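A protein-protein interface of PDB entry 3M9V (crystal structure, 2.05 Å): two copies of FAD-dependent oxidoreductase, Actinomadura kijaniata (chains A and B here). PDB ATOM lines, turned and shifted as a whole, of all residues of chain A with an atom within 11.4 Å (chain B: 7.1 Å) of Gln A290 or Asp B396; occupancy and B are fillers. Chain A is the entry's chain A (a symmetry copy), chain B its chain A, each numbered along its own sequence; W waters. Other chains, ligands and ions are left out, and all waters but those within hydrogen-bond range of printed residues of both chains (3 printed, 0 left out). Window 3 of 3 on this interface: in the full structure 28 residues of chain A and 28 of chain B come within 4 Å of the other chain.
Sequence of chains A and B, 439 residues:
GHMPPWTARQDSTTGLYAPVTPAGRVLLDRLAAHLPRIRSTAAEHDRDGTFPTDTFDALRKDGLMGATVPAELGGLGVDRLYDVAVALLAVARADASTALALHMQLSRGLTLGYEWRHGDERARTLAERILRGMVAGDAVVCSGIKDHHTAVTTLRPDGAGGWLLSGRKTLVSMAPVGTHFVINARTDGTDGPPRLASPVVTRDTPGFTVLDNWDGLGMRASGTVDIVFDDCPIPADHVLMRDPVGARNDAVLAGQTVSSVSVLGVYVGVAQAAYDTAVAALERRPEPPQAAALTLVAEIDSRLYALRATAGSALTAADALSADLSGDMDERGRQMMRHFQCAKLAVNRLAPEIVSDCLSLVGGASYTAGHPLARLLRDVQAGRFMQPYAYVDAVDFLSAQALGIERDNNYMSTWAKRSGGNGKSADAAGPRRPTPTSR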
ATOM      1  N   ALA A 278     -29.890 -20.411 -21.993  1.00  0.00           N
ATOM      2  CA  ALA A 278     -28.951 -21.063 -21.090  1.00  0.00           C
ATOM      3  C   ALA A 278     -28.416 -20.089 -20.049  1.00  0.00           C
ATOM      4  O   ALA A 278     -28.408 -20.416 -18.869  1.00  0.00           O
ATOM      5  CB  ALA A 278     -27.794 -21.707 -21.826  1.00  0.00           C
ATOM      6  N   ALA A 281     -31.047 -19.214 -17.520  1.00  0.00           N
ATOM      7  CA  ALA A 281     -31.161 -20.351 -16.607  1.00  0.00           C
ATOM      8  C   ALA A 281     -30.054 -20.374 -15.546  1.00  0.00           C
ATOM      9  O   ALA A 281     -30.314 -20.626 -14.363  1.00  0.00           O
ATOM     10  CB  ALA A 281     -31.280 -21.695 -17.344  1.00  0.00           C
ATOM     11  N   LEU A 282     -28.815 -20.065 -15.921  1.00  0.00           N
ATOM     12  CA  LEU A 282     -27.736 -20.136 -14.954  1.00  0.00           C
ATOM     13  C   LEU A 282     -27.847 -19.015 -13.931  1.00  0.00           C
ATOM     14  O   LEU A 282     -27.544 -19.213 -12.752  1.00  0.00           O
ATOM     15  CB  LEU A 282     -26.369 -20.057 -15.635  1.00  0.00           C
ATOM     16  CG  LEU A 282     -25.922 -21.367 -16.264  1.00  0.00           C
ATOM     17  CD1 LEU A 282     -24.781 -20.992 -17.200  1.00  0.00           C
ATOM     18  CD2 LEU A 282     -25.438 -22.292 -15.169  1.00  0.00           C
ATOM     19  N   GLU A 283     -28.256 -17.838 -14.397  1.00  0.00           N
ATOM     20  CA  GLU A 283     -28.408 -16.711 -13.491  1.00  0.00           C
ATOM     21  C   GLU A 283     -29.559 -16.866 -12.507  1.00  0.00           C
ATOM     22  O   GLU A 283     -29.584 -16.166 -11.503  1.00  0.00           O
ATOM     23  CB  GLU A 283     -28.523 -15.415 -14.284  1.00  0.00           C
ATOM     24  CG  GLU A 283     -27.387 -15.444 -15.280  1.00  0.00           C
ATOM     25  CD  GLU A 283     -27.089 -14.101 -15.893  1.00  0.00           C
ATOM     26  OE1 GLU A 283     -28.029 -13.335 -16.208  1.00  0.00           O
ATOM     27  OE2 GLU A 283     -25.881 -13.842 -16.059  1.00  0.00           O
ATOM     28  N   ARG A 285     -30.151 -19.383 -10.730  1.00  0.00           N
ATOM     29  CA  ARG A 285     -29.876 -20.382  -9.714  1.00  0.00           C
ATOM     30  C   ARG A 285     -29.208 -19.797  -8.473  1.00  0.00           C
ATOM     31  O   ARG A 285     -28.373 -18.903  -8.561  1.00  0.00           O
ATOM     32  CB  ARG A 285     -29.087 -21.543 -10.314  1.00  0.00           C
ATOM     33  CG  ARG A 285     -29.937 -22.314 -11.302  1.00  0.00           C
ATOM     34  CD  ARG A 285     -29.148 -23.363 -12.076  1.00  0.00           C
ATOM     35  NE  ARG A 285     -29.997 -23.962 -13.104  1.00  0.00           N
ATOM     36  CZ  ARG A 285     -29.573 -24.696 -14.131  1.00  0.00           C
ATOM     37  NH1 ARG A 285     -28.282 -24.945 -14.286  1.00  0.00           N
ATOM     38  NH2 ARG A 285     -30.446 -25.183 -15.004  1.00  0.00           N
ATOM     39  N   PRO A 286     -29.588 -20.301  -7.293  1.00  0.00           N
ATOM     40  CA  PRO A 286     -28.942 -19.892  -6.044  1.00  0.00           C
ATOM     41  C   PRO A 286     -27.450 -20.223  -6.052  1.00  0.00           C
ATOM     42  O   PRO A 286     -26.637 -19.395  -5.661  1.00  0.00           O
ATOM     43  CB  PRO A 286     -29.638 -20.750  -4.984  1.00  0.00           C
ATOM     44  CG  PRO A 286     -30.234 -21.919  -5.742  1.00  0.00           C
ATOM     45  CD  PRO A 286     -30.559 -21.395  -7.113  1.00  0.00           C
ATOM     46  N   GLU A 287     -27.087 -21.422  -6.495  1.00  0.00           N
ATOM     47  CA  GLU A 287     -25.681 -21.807  -6.546  1.00  0.00           C
ATOM     48  C   GLU A 287     -24.942 -21.115  -7.693  1.00  0.00           C
ATOM     49  O   GLU A 287     -25.509 -20.888  -8.763  1.00  0.00           O
ATOM     50  CB  GLU A 287     -25.556 -23.324  -6.692  1.00  0.00           C
ATOM     51  CG  GLU A 287     -25.480 -24.048  -5.355  1.00  0.00           C
ATOM     52  CD  GLU A 287     -26.800 -24.035  -4.600  1.00  0.00           C
ATOM     53  OE1 GLU A 287     -27.723 -24.810  -4.946  1.00  0.00           O
ATOM     54  OE2 GLU A 287     -26.901 -23.236  -3.641  1.00  0.00           O
ATOM     55  N   PRO A 288     -23.664 -20.782  -7.464  1.00  0.00           N
ATOM     56  CA  PRO A 288     -22.774 -20.293  -8.500  1.00  0.00           C
ATOM     57  C   PRO A 288     -22.472 -21.475  -9.429  1.00  0.00           C
ATOM     58  O   PRO A 288     -22.511 -22.625  -8.993  1.00  0.00           O
ATOM     59  CB  PRO A 288     -21.518 -19.884  -7.717  1.00  0.00           C
ATOM     60  CG  PRO A 288     -21.825 -20.085  -6.282  1.00  0.00           C
ATOM     61  CD  PRO A 288     -22.927 -21.097  -6.231  1.00  0.00           C
ATOM     62  N   PRO A 289     -22.223 -21.202 -10.712  1.00  0.00           N
ATOM     63  CA  PRO A 289     -22.049 -22.269 -11.696  1.00  0.00           C
ATOM     64  C   PRO A 289     -20.825 -23.135 -11.399  1.00  0.00           C
ATOM     65  O   PRO A 289     -19.784 -22.635 -10.986  1.00  0.00           O
ATOM     66  CB  PRO A 289     -21.877 -21.516 -13.026  1.00  0.00           C
ATOM     67  CG  PRO A 289     -22.311 -20.096 -12.763  1.00  0.00           C
ATOM     68  CD  PRO A 289     -22.124 -19.855 -11.300  1.00  0.00           C
ATOM     69  N   GLN A 290     -20.926 -24.431 -11.653  1.00  0.00           N
ATOM     70  CA  GLN A 290     -19.764 -25.306 -11.584  1.00  0.00           C
ATOM     71  C   GLN A 290     -18.674 -25.083 -12.640  1.00  0.00           C
ATOM     72  O   GLN A 290     -18.901 -24.397 -13.646  1.00  0.00           O
ATOM     73  CB  GLN A 290     -20.265 -26.741 -11.613  1.00  0.00           C
ATOM     74  CG  GLN A 290     -21.008 -27.032 -10.324  1.00  0.00           C
ATOM     75  CD  GLN A 290     -21.986 -28.150 -10.557  1.00  0.00           C
ATOM     76  OE1 GLN A 290     -23.131 -27.841 -10.933  1.00  0.00           O
ATOM     77  NE2 GLN A 290     -21.588 -29.319 -10.399  1.00  0.00           N
ATOM     78  N   ALA A 291     -17.494 -25.648 -12.382  1.00  0.00           N
ATOM     79  CA  ALA A 291     -16.323 -25.447 -13.221  1.00  0.00           C
ATOM     80  C   ALA A 291     -16.669 -25.789 -14.691  1.00  0.00           C
ATOM     81  O   ALA A 291     -16.349 -25.019 -15.596  1.00  0.00           O
ATOM     82  CB  ALA A 291     -15.241 -26.387 -12.736  1.00  0.00           C
ATOM     83  N   ALA A 292     -17.349 -26.907 -14.937  1.00  0.00           N
ATOM     84  CA  ALA A 292     -17.670 -27.261 -16.322  1.00  0.00           C
ATOM     85  C   ALA A 292     -18.663 -26.305 -16.970  1.00  0.00           C
ATOM     86  O   ALA A 292     -18.674 -26.175 -18.206  1.00  0.00           O
ATOM     87  CB  ALA A 292     -18.247 -28.658 -16.390  1.00  0.00           C
ATOM     88  N   ALA A 293     -19.507 -25.662 -16.157  1.00  0.00           N
ATOM     89  CA  ALA A 293     -20.515 -24.760 -16.711  1.00  0.00           C
ATOM     90  C   ALA A 293     -19.821 -23.471 -17.116  1.00  0.00           C
ATOM     91  O   ALA A 293     -20.153 -22.895 -18.159  1.00  0.00           O
ATOM     92  CB  ALA A 293     -21.687 -24.499 -15.728  1.00  0.00           C
ATOM     93  N   LEU A 294     -18.828 -23.040 -16.341  1.00  0.00           N
ATOM     94  CA  LEU A 294     -18.138 -21.783 -16.669  1.00  0.00           C
ATOM     95  C   LEU A 294     -17.376 -22.001 -17.969  1.00  0.00           C
ATOM     96  O   LEU A 294     -17.287 -21.108 -18.813  1.00  0.00           O
ATOM     97  CB  LEU A 294     -17.095 -21.429 -15.602  1.00  0.00           C
ATOM     98  CG  LEU A 294     -17.689 -21.021 -14.247  1.00  0.00           C
ATOM     99  CD1 LEU A 294     -16.539 -20.758 -13.278  1.00  0.00           C
ATOM    100  CD2 LEU A 294     -18.602 -19.813 -14.405  1.00  0.00           C
ATOM    101  N   THR A 295     -16.824 -23.198 -18.130  1.00  0.00           N
ATOM    102  CA  THR A 295     -15.978 -23.474 -19.300  1.00  0.00           C
ATOM    103  C   THR A 295     -16.870 -23.548 -20.544  1.00  0.00           C
ATOM    104  O   THR A 295     -16.565 -22.888 -21.530  1.00  0.00           O
ATOM    105  CB  THR A 295     -15.212 -24.794 -19.083  1.00  0.00           C
ATOM    106  OG1 THR A 295     -14.307 -24.634 -17.986  1.00  0.00           O
ATOM    107  CG2 THR A 295     -14.413 -25.217 -20.335  1.00  0.00           C
ATOM    108  N   LEU A 296     -17.987 -24.272 -20.496  1.00  0.00           N
ATOM    109  CA  LEU A 296     -19.024 -24.262 -21.542  1.00  0.00           C
ATOM    110  C   LEU A 296     -19.502 -22.864 -21.962  1.00  0.00           C
ATOM    111  O   LEU A 296     -19.584 -22.528 -23.151  1.00  0.00           O
ATOM    112  CB  LEU A 296     -20.235 -25.080 -21.074  1.00  0.00           C
ATOM    113  CG  LEU A 296     -20.096 -26.596 -21.306  1.00  0.00           C
ATOM    114  CD1 LEU A 296     -21.389 -27.215 -20.815  1.00  0.00           C
ATOM    115  CD2 LEU A 296     -19.915 -26.858 -22.797  1.00  0.00           C
ATOM    116  N   VAL A 297     -19.787 -22.024 -20.971  1.00  0.00           N
ATOM    117  CA  VAL A 297     -20.208 -20.665 -21.241  1.00  0.00           C
ATOM    118  C   VAL A 297     -19.129 -19.938 -22.049  1.00  0.00           C
ATOM    119  O   VAL A 297     -19.457 -19.233 -23.006  1.00  0.00           O
ATOM    120  CB  VAL A 297     -20.491 -19.878 -19.915  1.00  0.00           C
ATOM    121  CG1 VAL A 297     -20.555 -18.382 -20.223  1.00  0.00           C
ATOM    122  CG2 VAL A 297     -21.823 -20.401 -19.321  1.00  0.00           C
ATOM    123  N   ALA A 298     -17.855 -20.087 -21.685  1.00  0.00           N
ATOM    124  CA  ALA A 298     -16.807 -19.347 -22.389  1.00  0.00           C
ATOM    125  C   ALA A 298     -16.728 -19.962 -23.800  1.00  0.00           C
ATOM    126  O   ALA A 298     -16.578 -19.235 -24.774  1.00  0.00           O
ATOM    127  CB  ALA A 298     -15.443 -19.460 -21.653  1.00  0.00           C
ATOM    128  N   GLU A 299     -16.841 -21.277 -23.936  1.00  0.00           N
ATOM    129  CA  GLU A 299     -16.667 -21.910 -25.248  1.00  0.00           C
ATOM    130  C   GLU A 299     -17.800 -21.492 -26.188  1.00  0.00           C
ATOM    131  O   GLU A 299     -17.573 -21.145 -27.350  1.00  0.00           O
ATOM    132  CB  GLU A 299     -16.642 -23.448 -25.146  1.00  0.00           C
ATOM    133  CG  GLU A 299     -15.417 -24.053 -24.451  1.00  0.00           C
ATOM    134  CD  GLU A 299     -14.267 -24.220 -25.420  1.00  0.00           C
ATOM    135  OE1 GLU A 299     -14.520 -24.209 -26.660  1.00  0.00           O
ATOM    136  OE2 GLU A 299     -13.119 -24.335 -24.933  1.00  0.00           O
ATOM    137  N   SER A 360     -26.668 -28.992 -22.132  1.00  0.00           N
ATOM    138  CA  SER A 360     -25.807 -29.380 -21.022  1.00  0.00           C
ATOM    139  C   SER A 360     -25.833 -28.320 -19.913  1.00  0.00           C
ATOM    140  O   SER A 360     -25.783 -28.702 -18.750  1.00  0.00           O
ATOM    141  CB  SER A 360     -24.361 -29.573 -21.479  1.00  0.00           C
ATOM    142  OG  SER A 360     -24.341 -30.609 -22.438  1.00  0.00           O
ATOM    143  N   LEU A 361     -25.881 -27.024 -20.225  1.00  0.00           N
ATOM    144  CA  LEU A 361     -25.978 -26.009 -19.180  1.00  0.00           C
ATOM    145  C   LEU A 361     -27.295 -26.037 -18.403  1.00  0.00           C
ATOM    146  O   LEU A 361     -27.305 -25.893 -17.183  1.00  0.00           O
ATOM    147  CB  LEU A 361     -25.794 -24.609 -19.763  1.00  0.00           C
ATOM    148  CG  LEU A 361     -24.376 -24.440 -20.317  1.00  0.00           C
ATOM    149  CD1 LEU A 361     -24.217 -23.222 -21.199  1.00  0.00           C
ATOM    150  CD2 LEU A 361     -23.467 -24.378 -19.089  1.00  0.00           C
ATOM    151  N   VAL A 362     -28.428 -26.074 -19.093  1.00  0.00           N
ATOM    152  CA  VAL A 362     -29.715 -26.139 -18.433  1.00  0.00           C
ATOM    153  C   VAL A 362     -29.965 -27.478 -17.729  1.00  0.00           C
ATOM    154  O   VAL A 362     -30.591 -27.463 -16.676  1.00  0.00           O
ATOM    155  CB  VAL A 362     -30.827 -25.907 -19.454  1.00  0.00           C
ATOM    156  CG1 VAL A 362     -32.191 -26.095 -18.773  1.00  0.00           C
ATOM    157  CG2 VAL A 362     -30.654 -24.521 -20.064  1.00  0.00           C
ATOM    158  N   GLY A 363     -29.512 -28.592 -18.294  1.00  0.00           N
ATOM    159  CA  GLY A 363     -29.715 -29.939 -17.773  1.00  0.00           C
ATOM    160  C   GLY A 363     -31.086 -30.506 -18.126  1.00  0.00           C
ATOM    161  O   GLY A 363     -31.707 -30.003 -19.060  1.00  0.00           O
ATOM    162  N   GLY A 364     -31.582 -31.472 -17.344  1.00  0.00           N
ATOM    163  CA  GLY A 364     -32.703 -32.348 -17.686  1.00  0.00           C
ATOM    164  C   GLY A 364     -34.023 -31.697 -18.062  1.00  0.00           C
ATOM    165  O   GLY A 364     -34.762 -32.207 -18.916  1.00  0.00           O
ATOM    166  N   ALA B 390     -24.721 -36.393 -14.636  1.00  0.00           N
ATOM    167  CA  ALA B 390     -24.815 -35.520 -15.800  1.00  0.00           C
ATOM    168  C   ALA B 390     -23.470 -34.805 -15.998  1.00  0.00           C
ATOM    169  O   ALA B 390     -22.695 -34.693 -15.041  1.00  0.00           O
ATOM    170  CB  ALA B 390     -25.947 -34.505 -15.592  1.00  0.00           C
ATOM    171  N   TYR B 391     -23.204 -34.323 -17.216  1.00  0.00           N
ATOM    172  CA  TYR B 391     -21.912 -33.774 -17.623  1.00  0.00           C
ATOM    173  C   TYR B 391     -21.254 -32.859 -16.591  1.00  0.00           C
ATOM    174  O   TYR B 391     -20.120 -33.082 -16.181  1.00  0.00           O
ATOM    175  CB  TYR B 391     -22.008 -33.051 -18.974  1.00  0.00           C
ATOM    176  CG  TYR B 391     -20.701 -32.419 -19.363  1.00  0.00           C
ATOM    177  CD1 TYR B 391     -19.633 -33.206 -19.775  1.00  0.00           C
ATOM    178  CD2 TYR B 391     -20.530 -31.038 -19.342  1.00  0.00           C
ATOM    179  CE1 TYR B 391     -18.419 -32.658 -20.131  1.00  0.00           C
ATOM    180  CE2 TYR B 391     -19.306 -30.482 -19.708  1.00  0.00           C
ATOM    181  CZ  TYR B 391     -18.265 -31.289 -20.116  1.00  0.00           C
ATOM    182  OH  TYR B 391     -17.025 -30.794 -20.464  1.00  0.00           O
ATOM    183  N   VAL B 392     -21.963 -31.813 -16.190  1.00  0.00           N
ATOM    184  CA  VAL B 392     -21.435 -30.869 -15.205  1.00  0.00           C
ATOM    185  C   VAL B 392     -20.974 -31.491 -13.888  1.00  0.00           C
ATOM    186  O   VAL B 392     -19.855 -31.221 -13.422  1.00  0.00           O
ATOM    187  CB  VAL B 392     -22.349 -29.633 -15.049  1.00  0.00           C
ATOM    188  CG1 VAL B 392     -21.798 -28.745 -13.952  1.00  0.00           C
ATOM    189  CG2 VAL B 392     -22.364 -28.843 -16.397  1.00  0.00           C
ATOM    190  N   ASP B 393     -21.781 -32.380 -13.320  1.00  0.00           N
ATOM    191  CA  ASP B 393     -21.317 -33.151 -12.152  1.00  0.00           C
ATOM    192  C   ASP B 393     -20.264 -34.215 -12.433  1.00  0.00           C
ATOM    193  O   ASP B 393     -19.433 -34.501 -11.580  1.00  0.00           O
ATOM    194  CB  ASP B 393     -22.517 -33.841 -11.492  1.00  0.00           C
ATOM    195  CG  ASP B 393     -23.570 -32.829 -11.062  1.00  0.00           C
ATOM    196  OD1 ASP B 393     -23.193 -31.739 -10.599  1.00  0.00           O
ATOM    197  OD2 ASP B 393     -24.778 -33.088 -11.187  1.00  0.00           O
ATOM    198  N   ALA B 394     -20.287 -34.847 -13.602  1.00  0.00           N
ATOM    199  CA  ALA B 394     -19.260 -35.827 -13.917  1.00  0.00           C
ATOM    200  C   ALA B 394     -17.899 -35.131 -13.912  1.00  0.00           C
ATOM    201  O   ALA B 394     -16.877 -35.735 -13.576  1.00  0.00           O
ATOM    202  CB  ALA B 394     -19.496 -36.416 -15.339  1.00  0.00           C
ATOM    203  N   VAL B 395     -17.845 -33.885 -14.376  1.00  0.00           N
ATOM    204  CA  VAL B 395     -16.525 -33.275 -14.482  1.00  0.00           C
ATOM    205  C   VAL B 395     -15.989 -33.024 -13.053  1.00  0.00           C
ATOM    206  O   VAL B 395     -14.802 -33.232 -12.795  1.00  0.00           O
ATOM    207  CB  VAL B 395     -16.616 -31.962 -15.293  1.00  0.00           C
ATOM    208  CG1 VAL B 395     -15.444 -31.074 -14.956  1.00  0.00           C
ATOM    209  CG2 VAL B 395     -16.723 -32.301 -16.831  1.00  0.00           C
ATOM    210  N   ASP B 396     -16.858 -32.666 -12.108  1.00  0.00           N
ATOM    211  CA  ASP B 396     -16.354 -32.461 -10.729  1.00  0.00           C
ATOM    212  C   ASP B 396     -15.900 -33.789 -10.131  1.00  0.00           C
ATOM    213  O   ASP B 396     -14.893 -33.818  -9.442  1.00  0.00           O
ATOM    214  CB  ASP B 396     -17.444 -31.974  -9.753  1.00  0.00           C
ATOM    215  CG  ASP B 396     -17.862 -30.543  -9.996  1.00  0.00           C
ATOM    216  OD1 ASP B 396     -17.101 -29.762 -10.615  1.00  0.00           O
ATOM    217  OD2 ASP B 396     -19.001 -30.226  -9.605  1.00  0.00           O
ATOM    218  N   PHE B 397     -16.642 -34.872 -10.366  1.00  0.00           N
ATOM    219  CA  PHE B 397     -16.249 -36.193  -9.878  1.00  0.00           C
ATOM    220  C   PHE B 397     -14.905 -36.658 -10.458  1.00  0.00           C
ATOM    221  O   PHE B 397     -13.976 -37.027  -9.716  1.00  0.00           O
ATOM    222  CB  PHE B 397     -17.325 -37.246 -10.221  1.00  0.00           C
ATOM    223  CG  PHE B 397     -16.902 -38.664  -9.898  1.00  0.00           C
ATOM    224  CD1 PHE B 397     -16.841 -39.105  -8.582  1.00  0.00           C
ATOM    225  CD2 PHE B 397     -16.525 -39.543 -10.898  1.00  0.00           C
ATOM    226  CE1 PHE B 397     -16.426 -40.388  -8.281  1.00  0.00           C
ATOM    227  CE2 PHE B 397     -16.095 -40.837 -10.615  1.00  0.00           C
ATOM    228  CZ  PHE B 397     -16.046 -41.256  -9.306  1.00  0.00           C
ATOM    229  N   LEU B 398     -14.828 -36.690 -11.791  1.00  0.00           N
ATOM    230  CA  LEU B 398     -13.587 -37.089 -12.449  1.00  0.00           C
ATOM    231  C   LEU B 398     -12.376 -36.234 -12.113  1.00  0.00           C
ATOM    232  O   LEU B 398     -11.304 -36.787 -11.898  1.00  0.00           O
ATOM    233  CB  LEU B 398     -13.714 -37.190 -13.977  1.00  0.00           C
ATOM    234  CG  LEU B 398     -14.691 -38.296 -14.397  1.00  0.00           C
ATOM    235  CD1 LEU B 398     -14.994 -38.194 -15.894  1.00  0.00           C
ATOM    236  CD2 LEU B 398     -14.210 -39.688 -14.127  1.00  0.00           C
ATOM    237  N   SER B 399     -12.479 -34.912 -12.110  1.00  0.00           N
ATOM    238  CA  SER B 399     -11.270 -34.154 -11.822  1.00  0.00           C
ATOM    239  C   SER B 399     -10.893 -34.322 -10.349  1.00  0.00           C
ATOM    240  O   SER B 399      -9.712 -34.303 -10.024  1.00  0.00           O
ATOM    241  CB  SER B 399     -11.433 -32.683 -12.181  1.00  0.00           C
ATOM    242  OG  SER B 399     -12.546 -32.181 -11.466  1.00  0.00           O
ATOM    243  N   ALA B 400     -11.867 -34.521  -9.461  1.00  0.00           N
ATOM    244  CA  ALA B 400     -11.588 -34.781  -8.043  1.00  0.00           C
ATOM    245  C   ALA B 400     -10.783 -36.078  -7.879  1.00  0.00           C
ATOM    246  O   ALA B 400      -9.779 -36.131  -7.160  1.00  0.00           O
ATOM    247  CB  ALA B 400     -12.906 -34.836  -7.234  1.00  0.00           C
ATOM    248  N   GLN B 401     -11.207 -37.125  -8.573  1.00  0.00           N
ATOM    249  CA  GLN B 401     -10.554 -38.424  -8.497  1.00  0.00           C
ATOM    250  C   GLN B 401      -9.166 -38.317  -9.135  1.00  0.00           C
ATOM    251  O   GLN B 401      -8.222 -38.859  -8.586  1.00  0.00           O
ATOM    252  CB  GLN B 401     -11.324 -39.483  -9.296  1.00  0.00           C
ATOM    253  CG  GLN B 401     -12.668 -39.829  -8.697  1.00  0.00           C
ATOM    254  CD  GLN B 401     -12.528 -40.300  -7.266  1.00  0.00           C
ATOM    255  OE1 GLN B 401     -13.053 -39.685  -6.340  1.00  0.00           O
ATOM    256  NE2 GLN B 401     -11.818 -41.398  -7.074  1.00  0.00           N
ATOM    257  N   ALA B 402      -9.024 -37.655 -10.280  1.00  0.00           N
ATOM    258  CA  ALA B 402      -7.742 -37.674 -10.988  1.00  0.00           C
ATOM    259  C   ALA B 402      -6.712 -36.874 -10.197  1.00  0.00           C
ATOM    260  O   ALA B 402      -5.537 -37.190 -10.237  1.00  0.00           O
ATOM    261  CB  ALA B 402      -7.867 -37.087 -12.393  1.00  0.00           C
ATOM    262  N   ILE B 405      -8.242 -35.030  -5.078  1.00  0.00           N
ATOM    263  CA  ILE B 405      -8.899 -34.115  -4.158  1.00  0.00           C
ATOM    264  C   ILE B 405      -9.881 -34.880  -3.273  1.00  0.00           C
ATOM    265  O   ILE B 405     -11.075 -34.590  -3.290  1.00  0.00           O
ATOM    266  CB  ILE B 405      -9.709 -33.038  -4.889  1.00  0.00           C
ATOM    267  CG1 ILE B 405      -8.763 -32.012  -5.513  1.00  0.00           C
ATOM    268  CG2 ILE B 405     -10.705 -32.415  -3.915  1.00  0.00           C
ATOM    269  CD1 ILE B 405      -9.455 -31.088  -6.506  1.00  0.00           C
HETATM  270  O   HOH W   1     -17.247 -27.132  -9.826  1.00  0.00           O
HETATM  271  O   HOH W   2     -18.048 -29.015 -13.168  1.00  0.00           O
HETATM  272  O   HOH W   3     -24.630 -31.210 -17.309  1.00  0.00           O
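The side-chain carboxylate (OD1) of Asp B393 lies within hydrogen-bond range of the side-chain amide nitrogen (NE2) of Gln A290 (2.9 Å). OD2 of Asp B396 is in hydrogen-bond range of NE2 of Gln A290 (2.9 Å).
OG of Ser B399 lies within hydrogen-bond range of O of Val B395 (2.8 Å).
Gln A290 touches Val B392. CB of Ala A292 touches CE2 of Tyr B391 (3.9 Å). Ala A292 touches Val B395 (CB to CB, 3.8 Å).
Of the printed residues of chain B, Ala A292 touches Tyr B391 (3.9 Å) and Val B395 (3.8 Å). Ser A360 touches none of the printed residues of chain B. Of the printed residues of chain A, Tyr B391 touches Ala A292. No residue of chain A comes within 4 Å of Ala B394. Val B395 touches just one residue of chain A: Ala A292. Of chain A, only Gln A290 comes within 4 Å of Asp B396. Leu B398 touches none of the printed residues of chain A. No residue of chain A comes within 4 Å of Ser B399. No residue of chain A comes within 4 Å of Ala B400. The nearest residue of chain B that does not touch Gln A290 is Ala B394 (6.5 Å). The nearest printed residue of chain B that does not touch Ala A292 is Val B392 (4.1 Å).
Hydrophobic or aromatic side chains of chain A that line the printed part of chain B: Ala A292. Of the 14 printed residues of chain B, 5 touch a printed residue of chain A. Hydrophobic or aromatic side chains of chain B that line the printed part of chain A: Tyr B391, Val B392 and Val B395.
No position is printed for both chains.
Water W1 bridges OD1 of Asp B396 (2.7 Å) and N of Ala A291 (3.0 Å). Water W2 lies within hydrogen-bond range of the side-chain carboxylate of Asp B396 (2.8 Å), the backbone NH of Ala A292 (2.8 Å) and the backbone carbonyl oxygen of Val B392 (2.9 Å). Water W3 lies within hydrogen-bond range of the backbone NH (N) of Val B392 (3.0 Å), the backbone carbonyl oxygen (O) of Ser A360 (3.1 Å) and the backbone NH (N) of Tyr B391 (3.4 Å).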
